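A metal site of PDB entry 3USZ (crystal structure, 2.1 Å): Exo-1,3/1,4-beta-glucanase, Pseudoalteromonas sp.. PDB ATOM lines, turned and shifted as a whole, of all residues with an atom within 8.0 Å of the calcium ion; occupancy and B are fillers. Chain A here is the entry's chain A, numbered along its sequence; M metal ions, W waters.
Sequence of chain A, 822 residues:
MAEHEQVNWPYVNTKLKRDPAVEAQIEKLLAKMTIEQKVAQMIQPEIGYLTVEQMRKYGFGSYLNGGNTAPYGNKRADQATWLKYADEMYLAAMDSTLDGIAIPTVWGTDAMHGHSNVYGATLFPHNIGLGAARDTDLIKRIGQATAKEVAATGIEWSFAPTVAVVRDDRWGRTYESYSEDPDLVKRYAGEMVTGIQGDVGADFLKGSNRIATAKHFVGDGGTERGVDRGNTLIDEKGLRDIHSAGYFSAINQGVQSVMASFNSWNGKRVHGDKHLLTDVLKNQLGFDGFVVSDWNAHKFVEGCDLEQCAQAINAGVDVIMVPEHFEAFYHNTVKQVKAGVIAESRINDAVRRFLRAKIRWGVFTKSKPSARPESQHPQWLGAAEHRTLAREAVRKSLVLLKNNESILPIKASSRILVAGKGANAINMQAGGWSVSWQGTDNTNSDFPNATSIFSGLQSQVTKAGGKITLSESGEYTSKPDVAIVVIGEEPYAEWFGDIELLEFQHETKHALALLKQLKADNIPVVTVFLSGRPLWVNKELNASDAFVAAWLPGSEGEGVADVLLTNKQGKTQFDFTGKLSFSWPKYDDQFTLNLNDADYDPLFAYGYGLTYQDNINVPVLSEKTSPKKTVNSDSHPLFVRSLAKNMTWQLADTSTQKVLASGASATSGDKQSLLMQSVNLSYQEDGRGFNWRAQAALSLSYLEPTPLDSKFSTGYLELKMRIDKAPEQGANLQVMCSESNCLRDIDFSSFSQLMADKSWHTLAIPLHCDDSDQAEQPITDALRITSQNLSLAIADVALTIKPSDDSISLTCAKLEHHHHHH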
ATOM      1  N   VAL A 166     -18.029  30.456  -2.945  1.00  0.00           N
ATOM      2  CA  VAL A 166     -17.021  30.696  -1.898  1.00  0.00           C
ATOM      3  C   VAL A 166     -17.291  29.897  -0.627  1.00  0.00           C
ATOM      4  O   VAL A 166     -18.390  29.963  -0.071  1.00  0.00           O
ATOM      5  CB  VAL A 166     -16.899  32.205  -1.592  1.00  0.00           C
ATOM      6  CG1 VAL A 166     -16.052  32.436  -0.341  1.00  0.00           C
ATOM      7  CG2 VAL A 166     -16.273  32.925  -2.789  1.00  0.00           C
ATOM      8  N   ARG A 167     -16.282  29.146  -0.206  1.00  0.00           N
ATOM      9  CA  ARG A 167     -16.422  28.170   0.890  1.00  0.00           C
ATOM     10  C   ARG A 167     -15.683  28.576   2.168  1.00  0.00           C
ATOM     11  O   ARG A 167     -15.894  27.964   3.222  1.00  0.00           O
ATOM     12  CB  ARG A 167     -15.936  26.773   0.431  1.00  0.00           C
ATOM     13  CG  ARG A 167     -16.506  26.323  -0.918  1.00  0.00           C
ATOM     14  CD  ARG A 167     -17.987  26.007  -0.830  1.00  0.00           C
ATOM     15  NE  ARG A 167     -18.247  24.745  -0.131  1.00  0.00           N
ATOM     16  CZ  ARG A 167     -19.470  24.235   0.034  1.00  0.00           C
ATOM     17  NH1 ARG A 167     -20.522  24.887  -0.436  1.00  0.00           N
ATOM     18  NH2 ARG A 167     -19.641  23.076   0.660  1.00  0.00           N
ATOM     19  N   ASP A 168     -14.821  29.593   2.085  1.00  0.00           N
ATOM     20  CA  ASP A 168     -14.099  30.120   3.244  1.00  0.00           C
ATOM     21  C   ASP A 168     -14.072  31.649   3.143  1.00  0.00           C
ATOM     22  O   ASP A 168     -13.402  32.208   2.267  1.00  0.00           O
ATOM     23  CB  ASP A 168     -12.663  29.563   3.298  1.00  0.00           C
ATOM     24  CG  ASP A 168     -11.949  29.861   4.632  1.00  0.00           C
ATOM     25  OD1 ASP A 168     -12.141  30.945   5.227  1.00  0.00           O
ATOM     26  OD2 ASP A 168     -11.156  29.007   5.092  1.00  0.00           O
ATOM     27  N   ASP A 169     -14.805  32.309   4.036  1.00  0.00           N
ATOM     28  CA  ASP A 169     -15.024  33.763   3.937  1.00  0.00           C
ATOM     29  C   ASP A 169     -13.794  34.597   4.286  1.00  0.00           C
ATOM     30  O   ASP A 169     -13.837  35.824   4.224  1.00  0.00           O
ATOM     31  CB  ASP A 169     -16.189  34.194   4.844  1.00  0.00           C
ATOM     32  CG  ASP A 169     -17.497  33.522   4.478  1.00  0.00           C
ATOM     33  OD1 ASP A 169     -17.621  32.993   3.350  1.00  0.00           O
ATOM     34  OD2 ASP A 169     -18.398  33.524   5.341  1.00  0.00           O
ATOM     35  N   THR A 174     -14.531  37.315  -1.403  1.00  0.00           N
ATOM     36  CA  THR A 174     -15.825  36.728  -1.037  1.00  0.00           C
ATOM     37  C   THR A 174     -17.045  37.499  -1.570  1.00  0.00           C
ATOM     38  O   THR A 174     -18.020  36.899  -2.046  1.00  0.00           O
ATOM     39  CB  THR A 174     -15.923  36.523   0.496  1.00  0.00           C
ATOM     40  OG1 THR A 174     -14.912  35.603   0.914  1.00  0.00           O
ATOM     41  CG2 THR A 174     -17.295  35.971   0.876  1.00  0.00           C
ATOM     42  N   SER A 179     -22.914  33.379  -3.654  1.00  0.00           N
ATOM     43  CA  SER A 179     -23.320  32.414  -2.635  1.00  0.00           C
ATOM     44  C   SER A 179     -22.277  31.351  -2.316  1.00  0.00           C
ATOM     45  O   SER A 179     -21.391  31.071  -3.116  1.00  0.00           O
ATOM     46  CB  SER A 179     -24.610  31.699  -3.088  1.00  0.00           C
ATOM     47  OG  SER A 179     -25.003  30.719  -2.147  1.00  0.00           O
ATOM     48  N   GLU A 180     -22.395  30.745  -1.134  1.00  0.00           N
ATOM     49  CA  GLU A 180     -21.588  29.589  -0.787  1.00  0.00           C
ATOM     50  C   GLU A 180     -22.193  28.339  -1.426  1.00  0.00           C
ATOM     51  O   GLU A 180     -21.581  27.290  -1.445  1.00  0.00           O
ATOM     52  CB  GLU A 180     -21.524  29.404   0.739  1.00  0.00           C
ATOM     53  CG  GLU A 180     -22.821  28.877   1.347  1.00  0.00           C
ATOM     54  CD  GLU A 180     -22.867  28.990   2.879  1.00  0.00           C
ATOM     55  OE1 GLU A 180     -22.075  29.760   3.490  1.00  0.00           O
ATOM     56  OE2 GLU A 180     -23.704  28.299   3.479  1.00  0.00           O
ATOM     57  N   ASP A 181     -23.408  28.493  -1.957  1.00  0.00           N
ATOM     58  CA  ASP A 181     -24.200  27.374  -2.475  1.00  0.00           C
ATOM     59  C   ASP A 181     -24.116  27.274  -3.998  1.00  0.00           C
ATOM     60  O   ASP A 181     -24.548  28.190  -4.686  1.00  0.00           O
ATOM     61  CB  ASP A 181     -25.664  27.607  -2.070  1.00  0.00           C
ATOM     62  CG  ASP A 181     -26.621  26.572  -2.640  1.00  0.00           C
ATOM     63  OD1 ASP A 181     -26.187  25.444  -2.971  1.00  0.00           O
ATOM     64  OD2 ASP A 181     -27.838  26.883  -2.735  1.00  0.00           O
ATOM     65  N   PRO A 534     -20.228  37.595   5.873  1.00  0.00           N
ATOM     66  CA  PRO A 534     -20.546  37.482   7.299  1.00  0.00           C
ATOM     67  C   PRO A 534     -19.262  37.579   8.114  1.00  0.00           C
ATOM     68  O   PRO A 534     -18.196  37.181   7.643  1.00  0.00           O
ATOM     69  CB  PRO A 534     -21.130  36.063   7.422  1.00  0.00           C
ATOM     70  CG  PRO A 534     -21.664  35.755   6.051  1.00  0.00           C
ATOM     71  CD  PRO A 534     -20.682  36.422   5.107  1.00  0.00           C
ATOM     72  N   SER A 581     -27.310  34.159   1.752  1.00  0.00           N
ATOM     73  CA  SER A 581     -26.754  33.260   0.748  1.00  0.00           C
ATOM     74  C   SER A 581     -25.401  32.724   1.216  1.00  0.00           C
ATOM     75  O   SER A 581     -24.792  31.882   0.556  1.00  0.00           O
ATOM     76  CB  SER A 581     -26.605  33.979  -0.604  1.00  0.00           C
ATOM     77  OG  SER A 581     -25.680  35.041  -0.527  1.00  0.00           O
ATOM     78  N   PHE A 582     -24.942  33.241   2.364  1.00  0.00           N
ATOM     79  CA  PHE A 582     -23.776  32.748   3.092  1.00  0.00           C
ATOM     80  C   PHE A 582     -24.194  32.500   4.557  1.00  0.00           C
ATOM     81  O   PHE A 582     -24.957  33.293   5.121  1.00  0.00           O
ATOM     82  CB  PHE A 582     -22.636  33.762   3.069  1.00  0.00           C
ATOM     83  CG  PHE A 582     -21.902  33.850   1.742  1.00  0.00           C
ATOM     84  CD1 PHE A 582     -20.696  33.211   1.564  1.00  0.00           C
ATOM     85  CD2 PHE A 582     -22.439  34.580   0.683  1.00  0.00           C
ATOM     86  CE1 PHE A 582     -20.018  33.284   0.353  1.00  0.00           C
ATOM     87  CE2 PHE A 582     -21.775  34.667  -0.514  1.00  0.00           C
ATOM     88  CZ  PHE A 582     -20.567  34.018  -0.695  1.00  0.00           C
ATOM     89  N   SER A 583     -23.682  31.431   5.169  1.00  0.00           N
ATOM     90  CA  SER A 583     -23.999  31.105   6.564  1.00  0.00           C
ATOM     91  C   SER A 583     -23.315  32.056   7.545  1.00  0.00           C
ATOM     92  O   SER A 583     -22.136  32.372   7.361  1.00  0.00           O
ATOM     93  CB  SER A 583     -23.590  29.667   6.879  1.00  0.00           C
ATOM     94  OG  SER A 583     -24.336  28.739   6.091  1.00  0.00           O
ATOM     95  N   TRP A 584     -24.019  32.485   8.574  1.00  0.00           N
ATOM     96  CA  TRP A 584     -23.466  33.436   9.551  1.00  0.00           C
ATOM     97  C   TRP A 584     -22.925  32.717  10.774  1.00  0.00           C
ATOM     98  O   TRP A 584     -23.660  31.934  11.386  1.00  0.00           O
ATOM     99  CB  TRP A 584     -24.533  34.439   9.996  1.00  0.00           C
ATOM    100  CG  TRP A 584     -23.939  35.715  10.483  1.00  0.00           C
ATOM    101  CD1 TRP A 584     -23.345  35.953  11.710  1.00  0.00           C
ATOM    102  CD2 TRP A 584     -23.865  36.941   9.764  1.00  0.00           C
ATOM    103  NE1 TRP A 584     -22.918  37.262  11.777  1.00  0.00           N
ATOM    104  CE2 TRP A 584     -23.229  37.891  10.590  1.00  0.00           C
ATOM    105  CE3 TRP A 584     -24.288  37.346   8.488  1.00  0.00           C
ATOM    106  CZ2 TRP A 584     -22.998  39.203  10.182  1.00  0.00           C
ATOM    107  CZ3 TRP A 584     -24.067  38.653   8.087  1.00  0.00           C
ATOM    108  CH2 TRP A 584     -23.420  39.567   8.934  1.00  0.00           C
ATOM    109  N   PRO A 585     -21.656  32.980  11.134  1.00  0.00           N
ATOM    110  CA  PRO A 585     -20.946  32.249  12.190  1.00  0.00           C
ATOM    111  C   PRO A 585     -21.409  32.571  13.612  1.00  0.00           C
ATOM    112  O   PRO A 585     -21.693  33.724  13.945  1.00  0.00           O
ATOM    113  CB  PRO A 585     -19.492  32.672  11.987  1.00  0.00           C
ATOM    114  CG  PRO A 585     -19.600  34.056  11.408  1.00  0.00           C
ATOM    115  CD  PRO A 585     -20.793  33.995  10.499  1.00  0.00           C
ATOM    116  N   GLN A 590     -15.410  29.582  13.182  1.00  0.00           N
ATOM    117  CA  GLN A 590     -16.166  28.816  12.183  1.00  0.00           C
ATOM    118  C   GLN A 590     -15.810  29.261  10.768  1.00  0.00           C
ATOM    119  O   GLN A 590     -16.615  29.910  10.078  1.00  0.00           O
ATOM    120  CB  GLN A 590     -17.655  28.946  12.433  1.00  0.00           C
ATOM    121  CG  GLN A 590     -18.126  28.137  13.626  1.00  0.00           C
ATOM    122  CD  GLN A 590     -19.607  28.294  13.865  1.00  0.00           C
ATOM    123  OE1 GLN A 590     -20.124  29.419  13.931  1.00  0.00           O
ATOM    124  NE2 GLN A 590     -20.299  27.177  13.985  1.00  0.00           N
ATOM    125  N   PHE A 591     -14.601  28.897  10.334  1.00  0.00           N
ATOM    126  CA  PHE A 591     -14.064  29.417   9.081  1.00  0.00           C
ATOM    127  C   PHE A 591     -14.727  28.855   7.832  1.00  0.00           C
ATOM    128  O   PHE A 591     -14.912  29.553   6.830  1.00  0.00           O
ATOM    129  CB  PHE A 591     -12.561  29.198   9.014  1.00  0.00           C
ATOM    130  CG  PHE A 591     -11.800  29.876  10.122  1.00  0.00           C
ATOM    131  CD1 PHE A 591     -11.838  31.255  10.250  1.00  0.00           C
ATOM    132  CD2 PHE A 591     -11.045  29.140  11.021  1.00  0.00           C
ATOM    133  CE1 PHE A 591     -11.150  31.888  11.260  1.00  0.00           C
ATOM    134  CE2 PHE A 591     -10.345  29.765  12.030  1.00  0.00           C
ATOM    135  CZ  PHE A 591     -10.394  31.143  12.156  1.00  0.00           C
ATOM    136  N   THR A 592     -15.083  27.575   7.878  1.00  0.00           N
ATOM    137  CA  THR A 592     -15.689  26.938   6.726  1.00  0.00           C
ATOM    138  C   THR A 592     -17.073  26.407   7.101  1.00  0.00           C
ATOM    139  O   THR A 592     -17.271  25.205   7.253  1.00  0.00           O
ATOM    140  CB  THR A 592     -14.796  25.810   6.178  1.00  0.00           C
ATOM    141  OG1 THR A 592     -14.461  24.909   7.232  1.00  0.00           O
ATOM    142  CG2 THR A 592     -13.502  26.402   5.602  1.00  0.00           C
ATOM    143  N   LEU A 593     -18.012  27.318   7.241  1.00  0.00           N
ATOM    144  CA  LEU A 593     -19.355  27.013   7.697  1.00  0.00           C
ATOM    145  C   LEU A 593     -20.289  27.090   6.501  1.00  0.00           C
ATOM    146  O   LEU A 593     -20.634  28.177   6.051  1.00  0.00           O
ATOM    147  CB  LEU A 593     -19.770  28.038   8.748  1.00  0.00           C
ATOM    148  CG  LEU A 593     -21.194  28.001   9.320  1.00  0.00           C
ATOM    149  CD1 LEU A 593     -21.411  26.794  10.233  1.00  0.00           C
ATOM    150  CD2 LEU A 593     -21.445  29.309  10.049  1.00  0.00           C
ATOM    151  N   ASN A 594     -20.690  25.930   5.988  1.00  0.00           N
ATOM    152  CA  ASN A 594     -21.411  25.851   4.728  1.00  0.00           C
ATOM    153  C   ASN A 594     -22.644  24.982   4.781  1.00  0.00           C
ATOM    154  O   ASN A 594     -22.641  23.911   5.392  1.00  0.00           O
ATOM    155  CB  ASN A 594     -20.473  25.364   3.608  1.00  0.00           C
ATOM    156  CG  ASN A 594     -19.345  26.349   3.340  1.00  0.00           C
ATOM    157  OD1 ASN A 594     -19.576  27.536   3.138  1.00  0.00           O
ATOM    158  ND2 ASN A 594     -18.107  25.859   3.376  1.00  0.00           N
ATOM    159  N   LEU A 595     -23.706  25.450   4.119  1.00  0.00           N
ATOM    160  CA  LEU A 595     -24.941  24.709   3.938  1.00  0.00           C
ATOM    161  C   LEU A 595     -24.625  23.247   3.588  1.00  0.00           C
ATOM    162  O   LEU A 595     -23.732  22.990   2.786  1.00  0.00           O
ATOM    163  CB  LEU A 595     -25.743  25.361   2.814  1.00  0.00           C
ATOM    164  CG  LEU A 595     -26.876  24.584   2.175  1.00  0.00           C
ATOM    165  CD1 LEU A 595     -28.088  24.554   3.101  1.00  0.00           C
ATOM    166  CD2 LEU A 595     -27.233  25.193   0.828  1.00  0.00           C
ATOM    167  N   ASP A 597     -23.103  21.021   5.385  1.00  0.00           N
ATOM    168  CA  ASP A 597     -21.993  20.442   6.152  1.00  0.00           C
ATOM    169  C   ASP A 597     -22.520  19.408   7.156  1.00  0.00           C
ATOM    170  O   ASP A 597     -23.665  19.493   7.597  1.00  0.00           O
ATOM    171  CB  ASP A 597     -21.222  21.520   6.920  1.00  0.00           C
ATOM    172  CG  ASP A 597     -20.197  22.244   6.053  1.00  0.00           C
ATOM    173  OD1 ASP A 597     -20.017  21.870   4.871  1.00  0.00           O
ATOM    174  OD2 ASP A 597     -19.556  23.189   6.570  1.00  0.00           O
ATOM    175  N   TYR A 600     -23.064  21.284  11.203  1.00  0.00           N
ATOM    176  CA  TYR A 600     -23.550  22.590  10.760  1.00  0.00           C
ATOM    177  C   TYR A 600     -24.241  23.270  11.909  1.00  0.00           C
ATOM    178  O   TYR A 600     -25.398  22.976  12.198  1.00  0.00           O
ATOM    179  CB  TYR A 600     -24.507  22.435   9.578  1.00  0.00           C
ATOM    180  CG  TYR A 600     -24.939  23.736   8.916  1.00  0.00           C
ATOM    181  CD1 TYR A 600     -26.289  24.055   8.821  1.00  0.00           C
ATOM    182  CD2 TYR A 600     -24.013  24.626   8.371  1.00  0.00           C
ATOM    183  CE1 TYR A 600     -26.712  25.227   8.200  1.00  0.00           C
ATOM    184  CE2 TYR A 600     -24.425  25.802   7.743  1.00  0.00           C
ATOM    185  CZ  TYR A 600     -25.776  26.103   7.673  1.00  0.00           C
ATOM    186  OH  TYR A 600     -26.220  27.266   7.069  1.00  0.00           O
ATOM    187  N   TYR A 606     -28.025  29.511   6.279  1.00  0.00           N
ATOM    188  CA  TYR A 606     -28.333  29.795   4.879  1.00  0.00           C
ATOM    189  C   TYR A 606     -29.857  29.828   4.753  1.00  0.00           C
ATOM    190  O   TYR A 606     -30.536  28.958   5.266  1.00  0.00           O
ATOM    191  CB  TYR A 606     -27.739  28.694   3.990  1.00  0.00           C
ATOM    192  CG  TYR A 606     -28.028  28.835   2.511  1.00  0.00           C
ATOM    193  CD1 TYR A 606     -27.116  29.460   1.662  1.00  0.00           C
ATOM    194  CD2 TYR A 606     -29.195  28.313   1.956  1.00  0.00           C
ATOM    195  CE1 TYR A 606     -27.369  29.578   0.307  1.00  0.00           C
ATOM    196  CE2 TYR A 606     -29.458  28.430   0.599  1.00  0.00           C
ATOM    197  CZ  TYR A 606     -28.543  29.065  -0.214  1.00  0.00           C
ATOM    198  OH  TYR A 606     -28.786  29.185  -1.568  1.00  0.00           O
HETATM  199 CA    CA M   1     -19.888  29.598   4.268  1.00  0.00          CA
HETATM  200  O   HOH W   1     -20.105  31.689   5.491  1.00  0.00           O
HETATM  201  O   HOH W   2     -17.803  29.443   5.462  1.00  0.00           O
HETATM  202  O   HOH W   3     -18.547  30.689   2.603  1.00  0.00           O
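The backbone carbonyl oxygen (O) of Glu 180 sits at hydrogen-bond distance from the guanidinium group (NH1) of Arg 167, at 2.8 Å.
The backbone NH (N) of Glu 180 lies within hydrogen-bond range of the backbone carbonyl oxygen (O) of Ser 581 (3.1 Å).
The backbone NH (N) of Asn 594 is in hydrogen-bond range of the side-chain carboxylate (OD2) of Asp 597.
The side-chain amide nitrogen (ND2) of Asn 594 sits at hydrogen-bond distance from the backbone carbonyl oxygen (O) of Arg 167 (3.1 Å).
The side-chain carboxylate (OE2) of Glu 180 sits at hydrogen-bond distance from the side-chain hydroxyl (OG) of Ser 583 (2.7 Å).
The side-chain carboxylate (OE2) of Glu 180 sits at hydrogen-bond distance from the backbone NH (N) of Leu 595 (2.9 Å).
Water W2 lies within hydrogen-bond range of N of Leu 593 (2.8 Å), O of Phe 591 (3.2 Å) and O of Arg 167 (3.3 Å).
Water W1 bridges the side-chain carboxylate of Asp 169 and the backbone carbonyl oxygen of Ser 583.
Water W3 bridges the side-chain carboxylate (OD1) of Asp 169 (2.6 Å) and the backbone carbonyl oxygen (O) of Val 166 (2.8 Å).
OE1 of Glu 180 binds the calcium ion (2.3 Å).
The calcium ion is bound by the side-chain amide oxygen (OD1) of Asn 594.
The calcium ion is bound by O of Leu 593 (2.4 Å).
The calcium ion is bound by water W3.
Water W2 is bound to the calcium ion, at 2.4 Å.
The calcium ion is bound by water W1, 2.4 Å away.
The calcium ion has six donor atoms within binding distance.
Within 4 Å of the calcium ion: Glu 180, Leu 593 and Asn 594.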
